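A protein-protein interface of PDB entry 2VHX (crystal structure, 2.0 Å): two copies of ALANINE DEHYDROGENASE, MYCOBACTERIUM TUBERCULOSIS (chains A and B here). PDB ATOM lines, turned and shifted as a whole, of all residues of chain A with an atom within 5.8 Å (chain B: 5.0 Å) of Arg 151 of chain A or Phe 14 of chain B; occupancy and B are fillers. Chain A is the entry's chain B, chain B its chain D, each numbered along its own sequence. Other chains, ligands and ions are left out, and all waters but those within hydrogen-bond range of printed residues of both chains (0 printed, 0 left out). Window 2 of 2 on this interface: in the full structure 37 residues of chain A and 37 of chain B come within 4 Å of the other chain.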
ATOM      1  N   HIS A 148      27.227  10.726 -17.455  1.00  0.00           N
ATOM      2  CA  HIS A 148      26.088  11.603 -17.707  1.00  0.00           C
ATOM      3  C   HIS A 148      25.439  11.385 -19.076  1.00  0.00           C
ATOM      4  O   HIS A 148      24.350  11.833 -19.300  1.00  0.00           O
ATOM      5  CB  HIS A 148      26.520  13.035 -17.499  1.00  0.00           C
ATOM      6  CG  HIS A 148      26.853  13.333 -16.062  1.00  0.00           C
ATOM      7  ND1 HIS A 148      25.880  13.576 -15.107  1.00  0.00           N
ATOM      8  CD2 HIS A 148      28.039  13.356 -15.407  1.00  0.00           C
ATOM      9  CE1 HIS A 148      26.460  13.787 -13.933  1.00  0.00           C
ATOM     10  NE2 HIS A 148      27.770  13.644 -14.088  1.00  0.00           N
ATOM     11  N   LEU A 149      26.103  10.667 -19.976  1.00  0.00           N
ATOM     12  CA  LEU A 149      25.425  10.158 -21.192  1.00  0.00           C
ATOM     13  C   LEU A 149      24.330   9.112 -20.881  1.00  0.00           C
ATOM     14  O   LEU A 149      23.500   8.831 -21.714  1.00  0.00           O
ATOM     15  CB  LEU A 149      26.443   9.558 -22.165  1.00  0.00           C
ATOM     16  CG  LEU A 149      26.975  10.465 -23.264  1.00  0.00           C
ATOM     17  CD1 LEU A 149      28.078   9.690 -24.061  1.00  0.00           C
ATOM     18  CD2 LEU A 149      25.791  10.939 -24.172  1.00  0.00           C
ATOM     19  N   MET A 150      24.321   8.539 -19.683  1.00  0.00           N
ATOM     20  CA  MET A 150      23.227   7.645 -19.300  1.00  0.00           C
ATOM     21  C   MET A 150      21.899   8.371 -19.176  1.00  0.00           C
ATOM     22  O   MET A 150      21.835   9.447 -18.555  1.00  0.00           O
ATOM     23  CB  MET A 150      23.540   6.898 -18.017  1.00  0.00           C
ATOM     24  CG  MET A 150      24.912   6.256 -17.998  1.00  0.00           C
ATOM     25  SD  MET A 150      25.135   5.106 -16.616  1.00  0.00           S
ATOM     26  CE  MET A 150      24.958   6.142 -15.222  1.00  0.00           C
ATOM     27  N   ARG A 151      20.833   7.772 -19.734  1.00  0.00           N
ATOM     28  CA  ARG A 151      19.510   8.419 -19.750  1.00  0.00           C
ATOM     29  C   ARG A 151      19.027   8.729 -18.343  1.00  0.00           C
ATOM     30  O   ARG A 151      18.332   9.710 -18.113  1.00  0.00           O
ATOM     31  CB  ARG A 151      18.491   7.604 -20.567  1.00  0.00           C
ATOM     32  CG  ARG A 151      17.030   8.098 -20.558  1.00  0.00           C
ATOM     33  CD  ARG A 151      16.815   9.447 -21.250  1.00  0.00           C
ATOM     34  NE  ARG A 151      15.389   9.690 -21.526  1.00  0.00           N
ATOM     35  CZ  ARG A 151      14.483  10.137 -20.643  1.00  0.00           C
ATOM     36  NH1 ARG A 151      14.839  10.427 -19.390  1.00  0.00           N
ATOM     37  NH2 ARG A 151      13.210  10.300 -21.019  1.00  0.00           N
ATOM     38  N   THR A 152      19.458   7.919 -17.385  1.00  0.00           N
ATOM     39  CA  THR A 152      19.100   8.125 -15.980  1.00  0.00           C
ATOM     40  C   THR A 152      19.751   9.351 -15.340  1.00  0.00           C
ATOM     41  O   THR A 152      19.343   9.804 -14.222  1.00  0.00           O
ATOM     42  CB  THR A 152      19.493   6.935 -15.132  1.00  0.00           C
ATOM     43  OG1 THR A 152      20.892   6.678 -15.295  1.00  0.00           O
ATOM     44  CG2 THR A 152      18.638   5.701 -15.489  1.00  0.00           C
ATOM     45  N   GLN A 153      20.780   9.869 -16.005  1.00  0.00           N
ATOM     46  CA  GLN A 153      21.440  11.120 -15.576  1.00  0.00           C
ATOM     47  C   GLN A 153      20.941  12.319 -16.406  1.00  0.00           C
ATOM     48  O   GLN A 153      21.357  13.454 -16.213  1.00  0.00           O
ATOM     49  CB  GLN A 153      22.963  10.982 -15.618  1.00  0.00           C
ATOM     50  CG  GLN A 153      23.500   9.746 -14.881  1.00  0.00           C
ATOM     51  CD  GLN A 153      23.089   9.694 -13.431  1.00  0.00           C
ATOM     52  OE1 GLN A 153      23.317  10.641 -12.685  1.00  0.00           O
ATOM     53  NE2 GLN A 153      22.490   8.573 -13.012  1.00  0.00           N
ATOM     54  N   GLY A 154      19.992  12.061 -17.301  1.00  0.00           N
ATOM     55  CA  GLY A 154      19.453  13.130 -18.144  1.00  0.00           C
ATOM     56  C   GLY A 154      20.061  13.159 -19.552  1.00  0.00           C
ATOM     57  O   GLY A 154      19.600  13.926 -20.407  1.00  0.00           O
ATOM     58  N   GLY A 155      21.063  12.317 -19.802  1.00  0.00           N
ATOM     59  CA  GLY A 155      21.718  12.294 -21.104  1.00  0.00           C
ATOM     60  C   GLY A 155      20.970  11.472 -22.138  1.00  0.00           C
ATOM     61  O   GLY A 155      19.917  10.923 -21.880  1.00  0.00           O
ATOM     62  N   ARG A 156      21.557  11.355 -23.315  1.00  0.00           N
ATOM     63  CA  ARG A 156      20.871  10.756 -24.468  1.00  0.00           C
ATOM     64  C   ARG A 156      20.690   9.239 -24.308  1.00  0.00           C
ATOM     65  O   ARG A 156      19.852   8.613 -24.981  1.00  0.00           O
ATOM     66  CB  ARG A 156      21.672  11.084 -25.752  1.00  0.00           C
ATOM     67  CG  ARG A 156      20.978  10.691 -27.033  1.00  0.00           C
ATOM     68  CD  ARG A 156      21.748  11.245 -28.229  1.00  0.00           C
ATOM     69  NE  ARG A 156      21.202  10.820 -29.512  1.00  0.00           N
ATOM     70  CZ  ARG A 156      20.056  11.251 -30.046  1.00  0.00           C
ATOM     71  NH1 ARG A 156      19.243  12.119 -29.404  1.00  0.00           N
ATOM     72  NH2 ARG A 156      19.701  10.770 -31.233  1.00  0.00           N
ATOM     73  N   GLY A 157      21.502   8.634 -23.451  1.00  0.00           N
ATOM     74  CA  GLY A 157      21.369   7.217 -23.128  1.00  0.00           C
ATOM     75  C   GLY A 157      22.194   6.340 -24.091  1.00  0.00           C
ATOM     76  O   GLY A 157      21.714   5.312 -24.529  1.00  0.00           O
ATOM     77  N   VAL A 158      23.438   6.746 -24.369  1.00  0.00           N
ATOM     78  CA  VAL A 158      24.340   6.085 -25.353  1.00  0.00           C
ATOM     79  C   VAL A 158      25.585   5.539 -24.623  1.00  0.00           C
ATOM     80  O   VAL A 158      26.278   6.287 -23.963  1.00  0.00           O
ATOM     81  CB  VAL A 158      24.808   7.068 -26.407  1.00  0.00           C
ATOM     82  CG1 VAL A 158      25.717   6.356 -27.438  1.00  0.00           C
ATOM     83  CG2 VAL A 158      23.599   7.697 -27.128  1.00  0.00           C
ATOM     84  N   ASN B  12      11.753   3.852 -14.671  1.00  0.00           N
ATOM     85  CA  ASN B  12      13.065   3.959 -15.311  1.00  0.00           C
ATOM     86  C   ASN B  12      13.398   3.003 -16.467  1.00  0.00           C
ATOM     87  O   ASN B  12      14.567   2.797 -16.786  1.00  0.00           O
ATOM     88  CB  ASN B  12      14.195   3.903 -14.281  1.00  0.00           C
ATOM     89  CG  ASN B  12      14.187   5.086 -13.356  1.00  0.00           C
ATOM     90  OD1 ASN B  12      14.306   6.240 -13.791  1.00  0.00           O
ATOM     91  ND2 ASN B  12      14.038   4.808 -12.065  1.00  0.00           N
ATOM     92  N   GLU B  13      12.380   2.402 -17.062  1.00  0.00           N
ATOM     93  CA  GLU B  13      12.589   1.578 -18.232  1.00  0.00           C
ATOM     94  C   GLU B  13      12.292   2.451 -19.447  1.00  0.00           C
ATOM     95  O   GLU B  13      11.150   2.897 -19.635  1.00  0.00           O
ATOM     96  CB  GLU B  13      11.690   0.334 -18.186  1.00  0.00           C
ATOM     97  CG  GLU B  13      11.921  -0.557 -19.382  1.00  0.00           C
ATOM     98  CD  GLU B  13      13.390  -0.960 -19.546  1.00  0.00           C
ATOM     99  OE1 GLU B  13      14.086  -0.494 -20.502  1.00  0.00           O
ATOM    100  OE2 GLU B  13      13.856  -1.749 -18.707  1.00  0.00           O
ATOM    101  N   PHE B  14      13.321   2.710 -20.247  1.00  0.00           N
ATOM    102  CA  PHE B  14      13.243   3.581 -21.414  1.00  0.00           C
ATOM    103  C   PHE B  14      13.490   2.840 -22.746  1.00  0.00           C
ATOM    104  O   PHE B  14      13.523   3.453 -23.774  1.00  0.00           O
ATOM    105  CB  PHE B  14      14.330   4.658 -21.328  1.00  0.00           C
ATOM    106  CG  PHE B  14      14.272   5.509 -20.085  1.00  0.00           C
ATOM    107  CD1 PHE B  14      15.307   5.436 -19.123  1.00  0.00           C
ATOM    108  CD2 PHE B  14      13.222   6.406 -19.885  1.00  0.00           C
ATOM    109  CE1 PHE B  14      15.279   6.256 -17.961  1.00  0.00           C
ATOM    110  CE2 PHE B  14      13.187   7.219 -18.726  1.00  0.00           C
ATOM    111  CZ  PHE B  14      14.225   7.153 -17.782  1.00  0.00           C
ATOM    112  N   ARG B  15      13.724   1.546 -22.696  1.00  0.00           N
ATOM    113  CA  ARG B  15      13.958   0.763 -23.891  1.00  0.00           C
ATOM    114  C   ARG B  15      12.655   0.555 -24.650  1.00  0.00           C
ATOM    115  O   ARG B  15      11.584   0.834 -24.143  1.00  0.00           O
ATOM    116  CB  ARG B  15      14.592  -0.554 -23.507  1.00  0.00           C
ATOM    117  CG  ARG B  15      15.969  -0.321 -22.905  1.00  0.00           C
ATOM    118  CD  ARG B  15      16.615  -1.609 -22.518  1.00  0.00           C
ATOM    119  NE  ARG B  15      16.118  -2.009 -21.215  1.00  0.00           N
ATOM    120  CZ  ARG B  15      16.446  -3.136 -20.603  1.00  0.00           C
ATOM    121  NH1 ARG B  15      17.248  -4.020 -21.209  1.00  0.00           N
ATOM    122  NH2 ARG B  15      15.932  -3.388 -19.405  1.00  0.00           N
ATOM    123  N   VAL B  16      12.736   0.120 -25.894  1.00  0.00           N
ATOM    124  CA  VAL B  16      11.528  -0.217 -26.641  1.00  0.00           C
ATOM    125  C   VAL B  16      11.861  -1.492 -27.376  1.00  0.00           C
ATOM    126  O   VAL B  16      13.032  -1.748 -27.669  1.00  0.00           O
ATOM    127  CB  VAL B  16      11.052   0.956 -27.560  1.00  0.00           C
ATOM    128  CG1 VAL B  16      12.159   1.423 -28.517  1.00  0.00           C
ATOM    129  CG2 VAL B  16       9.759   0.575 -28.330  1.00  0.00           C
ATOM    130  N   GLY B  42      12.106   7.220 -25.194  1.00  0.00           N
ATOM    131  CA  GLY B  42      13.165   6.921 -24.224  1.00  0.00           C
ATOM    132  C   GLY B  42      14.462   6.504 -24.932  1.00  0.00           C
ATOM    133  O   GLY B  42      15.562   6.692 -24.414  1.00  0.00           O
ATOM    134  N   SER B  43      14.335   5.973 -26.142  1.00  0.00           N
ATOM    135  CA  SER B  43      15.472   5.441 -26.903  1.00  0.00           C
ATOM    136  C   SER B  43      15.814   6.359 -28.055  1.00  0.00           C
ATOM    137  O   SER B  43      16.506   5.950 -28.997  1.00  0.00           O
ATOM    138  CB  SER B  43      15.117   4.045 -27.422  1.00  0.00           C
ATOM    139  OG  SER B  43      14.974   3.153 -26.329  1.00  0.00           O
ATOM    140  N   ALA B 303      18.969  -0.750 -18.916  1.00  0.00           N
ATOM    141  CA  ALA B 303      17.928   0.279 -19.039  1.00  0.00           C
ATOM    142  C   ALA B 303      18.503   1.682 -19.059  1.00  0.00           C
ATOM    143  O   ALA B 303      17.878   2.565 -19.649  1.00  0.00           O
ATOM    144  CB  ALA B 303      16.817   0.153 -17.931  1.00  0.00           C
ATOM    145  N   SER B 304      19.673   1.903 -18.454  1.00  0.00           N
ATOM    146  CA  SER B 304      20.220   3.275 -18.363  1.00  0.00           C
ATOM    147  C   SER B 304      20.897   3.832 -19.614  1.00  0.00           C
ATOM    148  O   SER B 304      21.268   5.009 -19.631  1.00  0.00           O
ATOM    149  CB  SER B 304      21.179   3.410 -17.216  1.00  0.00           C
ATOM    150  OG  SER B 304      22.328   2.675 -17.466  1.00  0.00           O
ATOM    151  N   VAL B 305      21.096   2.965 -20.610  1.00  0.00           N
ATOM    152  CA  VAL B 305      21.621   3.330 -21.926  1.00  0.00           C
ATOM    153  C   VAL B 305      20.688   2.803 -23.035  1.00  0.00           C
ATOM    154  O   VAL B 305      21.078   2.017 -23.900  1.00  0.00           O
ATOM    155  CB  VAL B 305      23.092   2.873 -22.147  1.00  0.00           C
ATOM    156  CG1 VAL B 305      24.079   3.732 -21.322  1.00  0.00           C
ATOM    157  CG2 VAL B 305      23.277   1.384 -21.863  1.00  0.00           C
ATOM    158  N   PRO B 306      19.449   3.290 -23.047  1.00  0.00           N
ATOM    159  CA  PRO B 306      18.418   2.685 -23.905  1.00  0.00           C
ATOM    160  C   PRO B 306      18.651   2.861 -25.389  1.00  0.00           C
ATOM    161  O   PRO B 306      18.301   1.983 -26.158  1.00  0.00           O
ATOM    162  CB  PRO B 306      17.144   3.409 -23.480  1.00  0.00           C
ATOM    163  CG  PRO B 306      17.640   4.728 -22.966  1.00  0.00           C
ATOM    164  CD  PRO B 306      18.933   4.439 -22.286  1.00  0.00           C
ATOM    165  N   THR B 310      18.445  -0.781 -26.562  1.00  0.00           N
ATOM    166  CA  THR B 310      17.284  -1.073 -27.428  1.00  0.00           C
ATOM    167  C   THR B 310      17.755  -1.751 -28.718  1.00  0.00           C
ATOM    168  O   THR B 310      17.229  -2.764 -29.124  1.00  0.00           O
ATOM    169  CB  THR B 310      16.489   0.194 -27.800  1.00  0.00           C
ATOM    170  OG1 THR B 310      15.617   0.501 -26.723  1.00  0.00           O
ATOM    171  CG2 THR B 310      15.629  -0.019 -29.071  1.00  0.00           C
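The backbone carbonyl oxygen (O) of Pro 306 of chain B sits close to the side-chain hydroxyl (OG1) of Thr 310 of chain B (3.1 Å).
OG of Ser 43 of chain B sits at hydrogen-bond distance from O of Phe 14 of chain B (3.0 Å).
OG1 of Thr 152 of chain A sits at hydrogen-bond distance from NE2 of Gln 153 of chain A, 3.4 Å away.
O of Leu 149 of chain A sits at hydrogen-bond distance from N of Gly 157 of chain A.
O of Met 150 of chain A is in hydrogen-bond range of N of Gly 155 of chain A (3.2 Å).
Among the printed residues, merely in contact across the chains: Met 150 of chain A with Ser 304 of chain B (3.3 Å), Arg 151 of chain A with Phe 14 of chain B (3.5 Å), Arg 151 of chain A with Pro 306 of chain B (3.6 Å) and Thr 152 of chain A with Ser 304 of chain B (3.8 Å).
Hydrophobic or aromatic side chains of chain B that line the printed part of chain A: Phe 14, Val 305 and Pro 306.
Along chain B the printed residues that touch a printed residue of chain A span positions 14 to 306.
Hydrophobic or aromatic side chains of chain A that line the printed part of chain B: Met 150.
Among the printed residues, no Asp or Glu carboxylate lies within 4 Å of a Lys or Arg side-chain nitrogen of the other chain.
No position is printed for both chains.
Arg 151 of chain A touches just these residues of chain B: Phe 14, Ser 304 and Pro 306.
Phe 14 of chain B touches just one residue of chain A: Arg 151 (3.5 Å).
Printed residues of chain B within 4 Å of Met 150 of chain A: Ser 304 (3.3 Å).
Of the printed residues of chain B, Gly 157 of chain A touches Val 305 (3.1 Å) and Pro 306 (3.4 Å).
Of the printed residues of chain A, Val 305 of chain B touches Gly 157 (3.1 Å).
Of the printed residues of chain A, Ser 304 of chain B touches Met 150 (3.3 Å), Arg 151 (2.8 Å) and Thr 152 (3.8 Å).
Gly 42 of chain B touches none of the printed residues of chain A.
The nearest residue of chain B that does not touch Arg 151 of chain A is Gly 42 of chain B (4.2 Å).
The nearest residue of chain A that does not touch Phe 14 of chain B is Thr 152 of chain A (4.2 Å).
The nearest printed residue of chain A that does not touch Pro 306 of chain B is Arg 156 of chain A (4.9 Å).
The backbone carbonyl oxygen (O) of Gly 157 of chain A lies close to the backbone carbonyl oxygen (O) of Val 305 of chain B.
The backbone nitrogen (N) of Pro 306 of chain B sits close to the backbone carbonyl oxygen (O) of Gly 157 of chain A, 3.4 Å away.
N of Arg 151 of chain A is in hydrogen-bond range of O of Ser 304 of chain B.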
